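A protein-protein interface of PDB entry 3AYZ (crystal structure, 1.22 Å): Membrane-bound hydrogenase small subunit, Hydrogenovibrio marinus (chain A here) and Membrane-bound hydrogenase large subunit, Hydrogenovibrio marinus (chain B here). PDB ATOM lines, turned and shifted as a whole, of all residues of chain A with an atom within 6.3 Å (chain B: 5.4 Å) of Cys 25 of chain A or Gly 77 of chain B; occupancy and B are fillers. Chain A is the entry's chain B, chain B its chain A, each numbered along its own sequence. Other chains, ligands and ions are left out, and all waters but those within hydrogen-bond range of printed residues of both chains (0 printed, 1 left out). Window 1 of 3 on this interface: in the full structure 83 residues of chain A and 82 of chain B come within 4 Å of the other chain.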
ATOM      1  N   GLU A  22     -11.955 -11.667 -16.369  1.00  0.00           N
ATOM      2  CA  GLU A  22     -10.587 -11.270 -16.407  1.00  0.00           C
ATOM      3  C   GLU A  22      -9.679 -12.513 -16.309  1.00  0.00           C
ATOM      4  O   GLU A  22     -10.148 -13.580 -15.934  1.00  0.00           O
ATOM      5  CB  GLU A  22     -10.284 -10.420 -15.148  1.00  0.00           C
ATOM      6  CG  GLU A  22     -10.272 -11.296 -13.913  1.00  0.00           C
ATOM      7  CD  GLU A  22     -10.071 -10.655 -12.604  1.00  0.00           C
ATOM      8  OE1 GLU A  22      -9.325  -9.655 -12.573  1.00  0.00           O
ATOM      9  OE2 GLU A  22     -10.512 -11.112 -11.546  1.00  0.00           O
ATOM     10  N   CYS A  23      -8.384 -12.295 -16.520  1.00  0.00           N
ATOM     11  CA  CYS A  23      -7.404 -13.285 -16.205  1.00  0.00           C
ATOM     12  C   CYS A  23      -6.448 -12.832 -15.086  1.00  0.00           C
ATOM     13  O   CYS A  23      -5.645 -13.627 -14.603  1.00  0.00           O
ATOM     14  CB  CYS A  23      -6.557 -13.749 -17.425  1.00  0.00           C
ATOM     15  SG  CYS A  23      -5.173 -12.647 -17.807  1.00  0.00           S
ATOM     16  N   THR A  24      -6.549 -11.558 -14.682  1.00  0.00           N
ATOM     17  CA  THR A  24      -5.716 -10.966 -13.609  1.00  0.00           C
ATOM     18  C   THR A  24      -4.366 -10.505 -14.100  1.00  0.00           C
ATOM     19  O   THR A  24      -3.525 -10.020 -13.334  1.00  0.00           O
ATOM     20  CB  THR A  24      -5.679 -11.777 -12.312  1.00  0.00           C
ATOM     21  OG1 THR A  24      -7.025 -12.264 -12.096  1.00  0.00           O
ATOM     22  CG2 THR A  24      -5.285 -11.021 -11.065  1.00  0.00           C
ATOM     23  N   CYS A  25      -4.156 -10.489 -15.427  1.00  0.00           N
ATOM     24  CA  CYS A  25      -2.843 -10.080 -15.922  1.00  0.00           C
ATOM     25  C   CYS A  25      -2.588  -8.598 -15.654  1.00  0.00           C
ATOM     26  O   CYS A  25      -1.422  -8.238 -15.536  1.00  0.00           O
ATOM     27  CB  CYS A  25      -2.693 -10.365 -17.410  1.00  0.00           C
ATOM     28  SG  CYS A  25      -3.767  -9.613 -18.652  1.00  0.00           S
ATOM     29  N   CYS A  26      -3.611  -7.757 -15.660  1.00  0.00           N
ATOM     30  CA  CYS A  26      -3.364  -6.336 -15.465  1.00  0.00           C
ATOM     31  C   CYS A  26      -2.926  -6.072 -14.044  1.00  0.00           C
ATOM     32  O   CYS A  26      -1.992  -5.248 -13.839  1.00  0.00           O
ATOM     33  CB  CYS A  26      -4.588  -5.541 -15.871  1.00  0.00           C
ATOM     34  SG  CYS A  26      -5.125  -5.833 -17.564  1.00  0.00           S
ATOM     35  N   SER A  27      -3.516  -6.694 -13.029  1.00  0.00           N
ATOM     36  CA  SER A  27      -3.071  -6.584 -11.641  1.00  0.00           C
ATOM     37  C   SER A  27      -1.627  -7.073 -11.514  1.00  0.00           C
ATOM     38  O   SER A  27      -0.812  -6.453 -10.800  1.00  0.00           O
ATOM     39  CB  SER A  27      -3.944  -7.352 -10.671  1.00  0.00           C
ATOM     40  OG  SER A  27      -5.149  -6.703 -10.422  1.00  0.00           O
ATOM     41  N   GLU A  28      -1.346  -8.198 -12.146  1.00  0.00           N
ATOM     42  CA  GLU A  28       0.004  -8.699 -12.102  1.00  0.00           C
ATOM     43  C   GLU A  28       1.008  -7.726 -12.725  1.00  0.00           C
ATOM     44  O   GLU A  28       2.083  -7.487 -12.200  1.00  0.00           O
ATOM     45  CB  GLU A  28       0.045 -10.066 -12.778  1.00  0.00           C
ATOM     46  CG  GLU A  28      -0.596 -11.143 -11.930  1.00  0.00           C
ATOM     47  CD  GLU A  28       0.276 -11.653 -10.811  1.00  0.00           C
ATOM     48  OE1 GLU A  28       1.455 -11.311 -10.641  1.00  0.00           O
ATOM     49  OE2 GLU A  28      -0.240 -12.562 -10.109  1.00  0.00           O
ATOM     50  N   SER A  29       0.658  -7.197 -13.902  1.00  0.00           N
ATOM     51  CA  SER A  29       1.549  -6.226 -14.513  1.00  0.00           C
ATOM     52  C   SER A  29       1.807  -5.058 -13.606  1.00  0.00           C
ATOM     53  O   SER A  29       2.964  -4.606 -13.457  1.00  0.00           O
ATOM     54  CB  SER A  29       1.019  -5.772 -15.875  1.00  0.00           C
ATOM     55  OG  SER A  29       2.079  -5.114 -16.507  1.00  0.00           O
ATOM     56  N   PHE A  30       0.782  -4.535 -12.973  1.00  0.00           N
ATOM     57  CA  PHE A  30       0.929  -3.360 -12.114  1.00  0.00           C
ATOM     58  C   PHE A  30       1.992  -3.547 -11.061  1.00  0.00           C
ATOM     59  O   PHE A  30       2.819  -2.668 -10.857  1.00  0.00           O
ATOM     60  CB  PHE A  30      -0.464  -3.094 -11.466  1.00  0.00           C
ATOM     61  CG  PHE A  30      -0.509  -1.863 -10.589  1.00  0.00           C
ATOM     62  CD1 PHE A  30      -0.690  -0.617 -11.186  1.00  0.00           C
ATOM     63  CD2 PHE A  30      -0.413  -1.979  -9.237  1.00  0.00           C
ATOM     64  CE1 PHE A  30      -0.864   0.527 -10.424  1.00  0.00           C
ATOM     65  CE2 PHE A  30      -0.546  -0.834  -8.442  1.00  0.00           C
ATOM     66  CZ  PHE A  30      -0.715   0.396  -9.032  1.00  0.00           C
ATOM     67  N   ARG A  32       4.584  -5.309 -11.221  1.00  0.00           N
ATOM     68  CA  ARG A  32       5.935  -5.389 -11.790  1.00  0.00           C
ATOM     69  C   ARG A  32       6.600  -4.038 -11.893  1.00  0.00           C
ATOM     70  O   ARG A  32       7.785  -3.960 -12.229  1.00  0.00           O
ATOM     71  CB  ARG A  32       5.923  -5.999 -13.198  1.00  0.00           C
ATOM     72  CG  ARG A  32       5.277  -7.368 -13.316  1.00  0.00           C
ATOM     73  CD  ARG A  32       5.990  -8.464 -12.468  1.00  0.00           C
ATOM     74  NE  ARG A  32       5.324  -9.702 -12.834  1.00  0.00           N
ATOM     75  CZ  ARG A  32       4.238 -10.278 -12.341  1.00  0.00           C
ATOM     76  NH1 ARG A  32       3.803  -9.857 -11.119  1.00  0.00           N
ATOM     77  NH2 ARG A  32       3.573 -11.246 -12.870  1.00  0.00           N
ATOM     78  N   GLU A  82     -10.531  -3.679 -13.993  1.00  0.00           N
ATOM     79  CA  GLU A  82      -9.876  -4.785 -14.658  1.00  0.00           C
ATOM     80  C   GLU A  82     -10.961  -5.755 -15.065  1.00  0.00           C
ATOM     81  O   GLU A  82     -11.886  -6.034 -14.311  1.00  0.00           O
ATOM     82  CB  GLU A  82      -8.846  -5.387 -13.742  1.00  0.00           C
ATOM     83  CG  GLU A  82      -8.057  -6.609 -14.306  1.00  0.00           C
ATOM     84  CD  GLU A  82      -6.889  -6.973 -13.386  1.00  0.00           C
ATOM     85  OE1 GLU A  82      -6.751  -6.354 -12.289  1.00  0.00           O
ATOM     86  OE2 GLU A  82      -6.097  -7.824 -13.746  1.00  0.00           O
ATOM     87  N   GLY A 157      -3.919  -3.088 -23.758  1.00  0.00           N
ATOM     88  CA  GLY A 157      -2.835  -4.048 -23.781  1.00  0.00           C
ATOM     89  C   GLY A 157      -3.207  -5.231 -22.918  1.00  0.00           C
ATOM     90  O   GLY A 157      -4.019  -5.121 -21.962  1.00  0.00           O
ATOM     91  N   CYS A 158      -2.616  -6.364 -23.220  1.00  0.00           N
ATOM     92  CA  CYS A 158      -2.969  -7.627 -22.568  1.00  0.00           C
ATOM     93  C   CYS A 158      -1.690  -8.244 -21.995  1.00  0.00           C
ATOM     94  O   CYS A 158      -1.091  -9.145 -22.554  1.00  0.00           O
ATOM     95  CB  CYS A 158      -3.653  -8.562 -23.488  1.00  0.00           C
ATOM     96  SG  CYS A 158      -4.298 -10.017 -22.676  1.00  0.00           S
ATOM     97  N   PRO A 159      -1.246  -7.809 -20.809  1.00  0.00           N
ATOM     98  CA  PRO A 159      -1.693  -6.587 -20.120  1.00  0.00           C
ATOM     99  C   PRO A 159      -0.963  -5.368 -20.641  1.00  0.00           C
ATOM    100  O   PRO A 159      -0.076  -5.458 -21.503  1.00  0.00           O
ATOM    101  CB  PRO A 159      -1.276  -6.886 -18.692  1.00  0.00           C
ATOM    102  CG  PRO A 159       0.014  -7.675 -18.829  1.00  0.00           C
ATOM    103  CD  PRO A 159      -0.122  -8.429 -20.140  1.00  0.00           C
ATOM    104  N   PRO A 160      -1.280  -4.176 -20.118  1.00  0.00           N
ATOM    105  CA  PRO A 160      -0.435  -2.994 -20.372  1.00  0.00           C
ATOM    106  C   PRO A 160       0.921  -3.181 -19.701  1.00  0.00           C
ATOM    107  O   PRO A 160       1.065  -3.925 -18.735  1.00  0.00           O
ATOM    108  CB  PRO A 160      -1.215  -1.839 -19.696  1.00  0.00           C
ATOM    109  CG  PRO A 160      -2.561  -2.389 -19.400  1.00  0.00           C
ATOM    110  CD  PRO A 160      -2.372  -3.839 -19.202  1.00  0.00           C
ATOM    111  N   MET A 165       1.122   1.709 -16.623  1.00  0.00           N
ATOM    112  CA  MET A 165       0.047   1.734 -15.633  1.00  0.00           C
ATOM    113  C   MET A 165       0.400   2.672 -14.485  1.00  0.00           C
ATOM    114  O   MET A 165      -0.414   3.564 -14.138  1.00  0.00           O
ATOM    115  CB  MET A 165      -0.215   0.338 -15.085  1.00  0.00           C
ATOM    116  CG  MET A 165      -0.631  -0.664 -16.100  1.00  0.00           C
ATOM    117  SD  MET A 165      -0.950  -2.317 -15.452  1.00  0.00           S
ATOM    118  CE  MET A 165      -2.555  -2.091 -14.751  1.00  0.00           C
ATOM    119  N   GLU B  73      -3.349 -18.874 -23.191  1.00  0.00           N
ATOM    120  CA  GLU B  73      -2.509 -18.214 -22.203  1.00  0.00           C
ATOM    121  C   GLU B  73      -3.324 -17.243 -21.352  1.00  0.00           C
ATOM    122  O   GLU B  73      -3.082 -17.127 -20.131  1.00  0.00           O
ATOM    123  CB  GLU B  73      -1.353 -17.487 -22.890  1.00  0.00           C
ATOM    124  CG  GLU B  73      -0.241 -17.036 -21.950  1.00  0.00           C
ATOM    125  CD  GLU B  73       0.915 -16.404 -22.643  1.00  0.00           C
ATOM    126  OE1 GLU B  73       0.686 -15.728 -23.641  1.00  0.00           O
ATOM    127  OE2 GLU B  73       2.068 -16.656 -22.176  1.00  0.00           O
ATOM    128  N   ILE B  75      -6.227 -17.600 -20.351  1.00  0.00           N
ATOM    129  CA  ILE B  75      -6.992 -18.191 -19.257  1.00  0.00           C
ATOM    130  C   ILE B  75      -6.578 -17.575 -17.924  1.00  0.00           C
ATOM    131  O   ILE B  75      -7.389 -17.368 -17.034  1.00  0.00           O
ATOM    132  CB  ILE B  75      -6.920 -19.717 -19.262  1.00  0.00           C
ATOM    133  CG1 ILE B  75      -7.668 -20.286 -20.445  1.00  0.00           C
ATOM    134  CG2 ILE B  75      -7.399 -20.348 -17.969  1.00  0.00           C
ATOM    135  CD1 ILE B  75      -7.405 -21.767 -20.673  1.00  0.00           C
ATOM    136  N   CYS B  76      -5.294 -17.230 -17.800  1.00  0.00           N
ATOM    137  CA  CYS B  76      -4.788 -16.842 -16.494  1.00  0.00           C
ATOM    138  C   CYS B  76      -3.505 -16.055 -16.562  1.00  0.00           C
ATOM    139  O   CYS B  76      -2.528 -16.445 -17.155  1.00  0.00           O
ATOM    140  CB  CYS B  76      -4.503 -18.021 -15.665  1.00  0.00           C
ATOM    141  SG  CYS B  76      -4.343 -17.429 -13.937  1.00  0.00           S
ATOM    142  N   GLY B  77      -3.543 -14.884 -15.903  1.00  0.00           N
ATOM    143  CA  GLY B  77      -2.391 -14.005 -15.816  1.00  0.00           C
ATOM    144  C   GLY B  77      -1.520 -14.203 -14.599  1.00  0.00           C
ATOM    145  O   GLY B  77      -0.448 -13.606 -14.559  1.00  0.00           O
ATOM    146  N   VAL B  78      -1.965 -15.051 -13.697  1.00  0.00           N
ATOM    147  CA  VAL B  78      -1.202 -15.410 -12.477  1.00  0.00           C
ATOM    148  C   VAL B  78      -0.300 -16.562 -12.873  1.00  0.00           C
ATOM    149  O   VAL B  78       0.936 -16.423 -12.837  1.00  0.00           O
ATOM    150  CB  VAL B  78      -2.153 -15.626 -11.324  1.00  0.00           C
ATOM    151  CG1 VAL B  78      -1.372 -16.037 -10.102  1.00  0.00           C
ATOM    152  CG2 VAL B  78      -3.068 -14.443 -11.007  1.00  0.00           C
ATOM    153  N   CYS B  79      -0.877 -17.663 -13.334  1.00  0.00           N
ATOM    154  CA  CYS B  79      -0.100 -18.794 -13.866  1.00  0.00           C
ATOM    155  C   CYS B  79       0.179 -18.538 -15.345  1.00  0.00           C
ATOM    156  O   CYS B  79      -0.049 -19.352 -16.224  1.00  0.00           O
ATOM    157  CB  CYS B  79      -0.843 -20.132 -13.610  1.00  0.00           C
ATOM    158  SG  CYS B  79      -2.471 -20.345 -14.292  1.00  0.00           S
ATOM    159  N   THR B  80       0.804 -17.394 -15.615  1.00  0.00           N
ATOM    160  CA  THR B  80       0.991 -16.909 -16.969  1.00  0.00           C
ATOM    161  C   THR B  80       2.070 -17.711 -17.669  1.00  0.00           C
ATOM    162  O   THR B  80       3.203 -17.799 -17.248  1.00  0.00           O
ATOM    163  CB  THR B  80       1.249 -15.415 -16.957  1.00  0.00           C
ATOM    164  OG1 THR B  80       1.385 -15.086 -18.310  1.00  0.00           O
ATOM    165  CG2 THR B  80       2.524 -14.994 -16.304  1.00  0.00           C
ATOM    166  N   PRO B 229       3.459 -10.115 -17.470  1.00  0.00           N
ATOM    167  CA  PRO B 229       2.749 -11.345 -17.871  1.00  0.00           C
ATOM    168  C   PRO B 229       2.670 -11.556 -19.369  1.00  0.00           C
ATOM    169  O   PRO B 229       2.847 -10.705 -20.202  1.00  0.00           O
ATOM    170  CB  PRO B 229       1.332 -11.079 -17.327  1.00  0.00           C
ATOM    171  CG  PRO B 229       1.512 -10.164 -16.150  1.00  0.00           C
ATOM    172  CD  PRO B 229       2.627  -9.265 -16.587  1.00  0.00           C
ATOM    173  N   HIS B 230       2.344 -12.810 -19.685  1.00  0.00           N
ATOM    174  CA  HIS B 230       1.939 -13.346 -20.992  1.00  0.00           C
ATOM    175  C   HIS B 230       3.118 -13.380 -21.985  1.00  0.00           C
ATOM    176  O   HIS B 230       3.039 -12.810 -23.083  1.00  0.00           O
ATOM    177  CB  HIS B 230       0.704 -12.680 -21.538  1.00  0.00           C
ATOM    178  CG  HIS B 230      -0.535 -12.933 -20.752  1.00  0.00           C
ATOM    179  ND1 HIS B 230      -0.771 -14.097 -20.082  1.00  0.00           N
ATOM    180  CD2 HIS B 230      -1.634 -12.157 -20.633  1.00  0.00           C
ATOM    181  CE1 HIS B 230      -1.963 -14.044 -19.546  1.00  0.00           C
ATOM    182  NE2 HIS B 230      -2.542 -12.879 -19.846  1.00  0.00           N
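The backbone NH (N) of Gly 77 of chain B lies within hydrogen-bond range of the backbone carbonyl oxygen (O) of Cys 23 of chain A (2.8 Å). A ring nitrogen (NE2) of His 230 of chain B lies close to the side-chain sulfur (SG) of Cys 23 of chain A. The side-chain sulfur of Cys 25 of chain A sits close to a ring nitrogen (NE2) of His 230 of chain B (3.7 Å).
SG of Cys 76 of chain B sits close to N of Val 78 of chain B, at 3.4 Å. OG1 of Thr 80 of chain B sits at hydrogen-bond distance from N of His 230 of chain B (2.8 Å). OE1 of Glu 28 of chain A is in salt-bridge range of NH1 of Arg 32 of chain A (2.8 Å). The side-chain hydroxyl of Ser 29 of chain A is in hydrogen-bond range of the backbone carbonyl oxygen of Pro 160 of chain A (2.7 Å).
Cys 23 of chain A touches Ile 75 of chain B (CB to O, 3.7 Å). CA of Cys 76 of chain B touches CB of Cys 23 of chain A, at 3.7 Å. Thr 24 of chain A touches Val 78 of chain B. Cys 25 of chain A touches Gly 77 of chain B (CA to CA, 3.95 Å). Pro 229 of chain B touches Cys 25 of chain A. Glu 28 of chain A touches Gly 77 of chain B (CG to O, 3.6 Å). Val 78 of chain B touches Glu 28 of chain A (CG2 to OE2, 3.5 Å). Pro 229 of chain B touches Glu 28 of chain A. His 230 of chain B touches Cys 158 of chain A (CD2 to O, 3.6 Å). Pro 229 of chain B touches Pro 159 of chain A.
Gly 77 of chain B touches three residues of chain A. Printed residues of chain A within 4 Å of His 230 of chain B: Cys 23, Cys 25 and Cys 158. Of the printed residues of chain A, Ile 75 of chain B touches Cys 23. Of the printed residues of chain B, Cys 158 of chain A touches His 230. Pro 160 of chain A touches none of the printed residues of chain B. The nearest residue of chain A that does not touch Gly 77 of chain B is Thr 24 of chain A (4.4 Å). The nearest printed residue of chain B that does not touch Ser 29 of chain A is Gly 77 of chain B (6.5 Å).
Of the 9 printed residues of chain B, 6 touch a printed residue of chain A. Hydrophobic or aromatic side chains of chain B within 4 Å of the printed part of chain A: Val 78, Pro 229 and His 230. Printed residues of chain A that touch a printed residue of chain B: Cys 23, Thr 24, Cys 25, Glu 28, Ser 29, Cys 158 and Pro 159.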
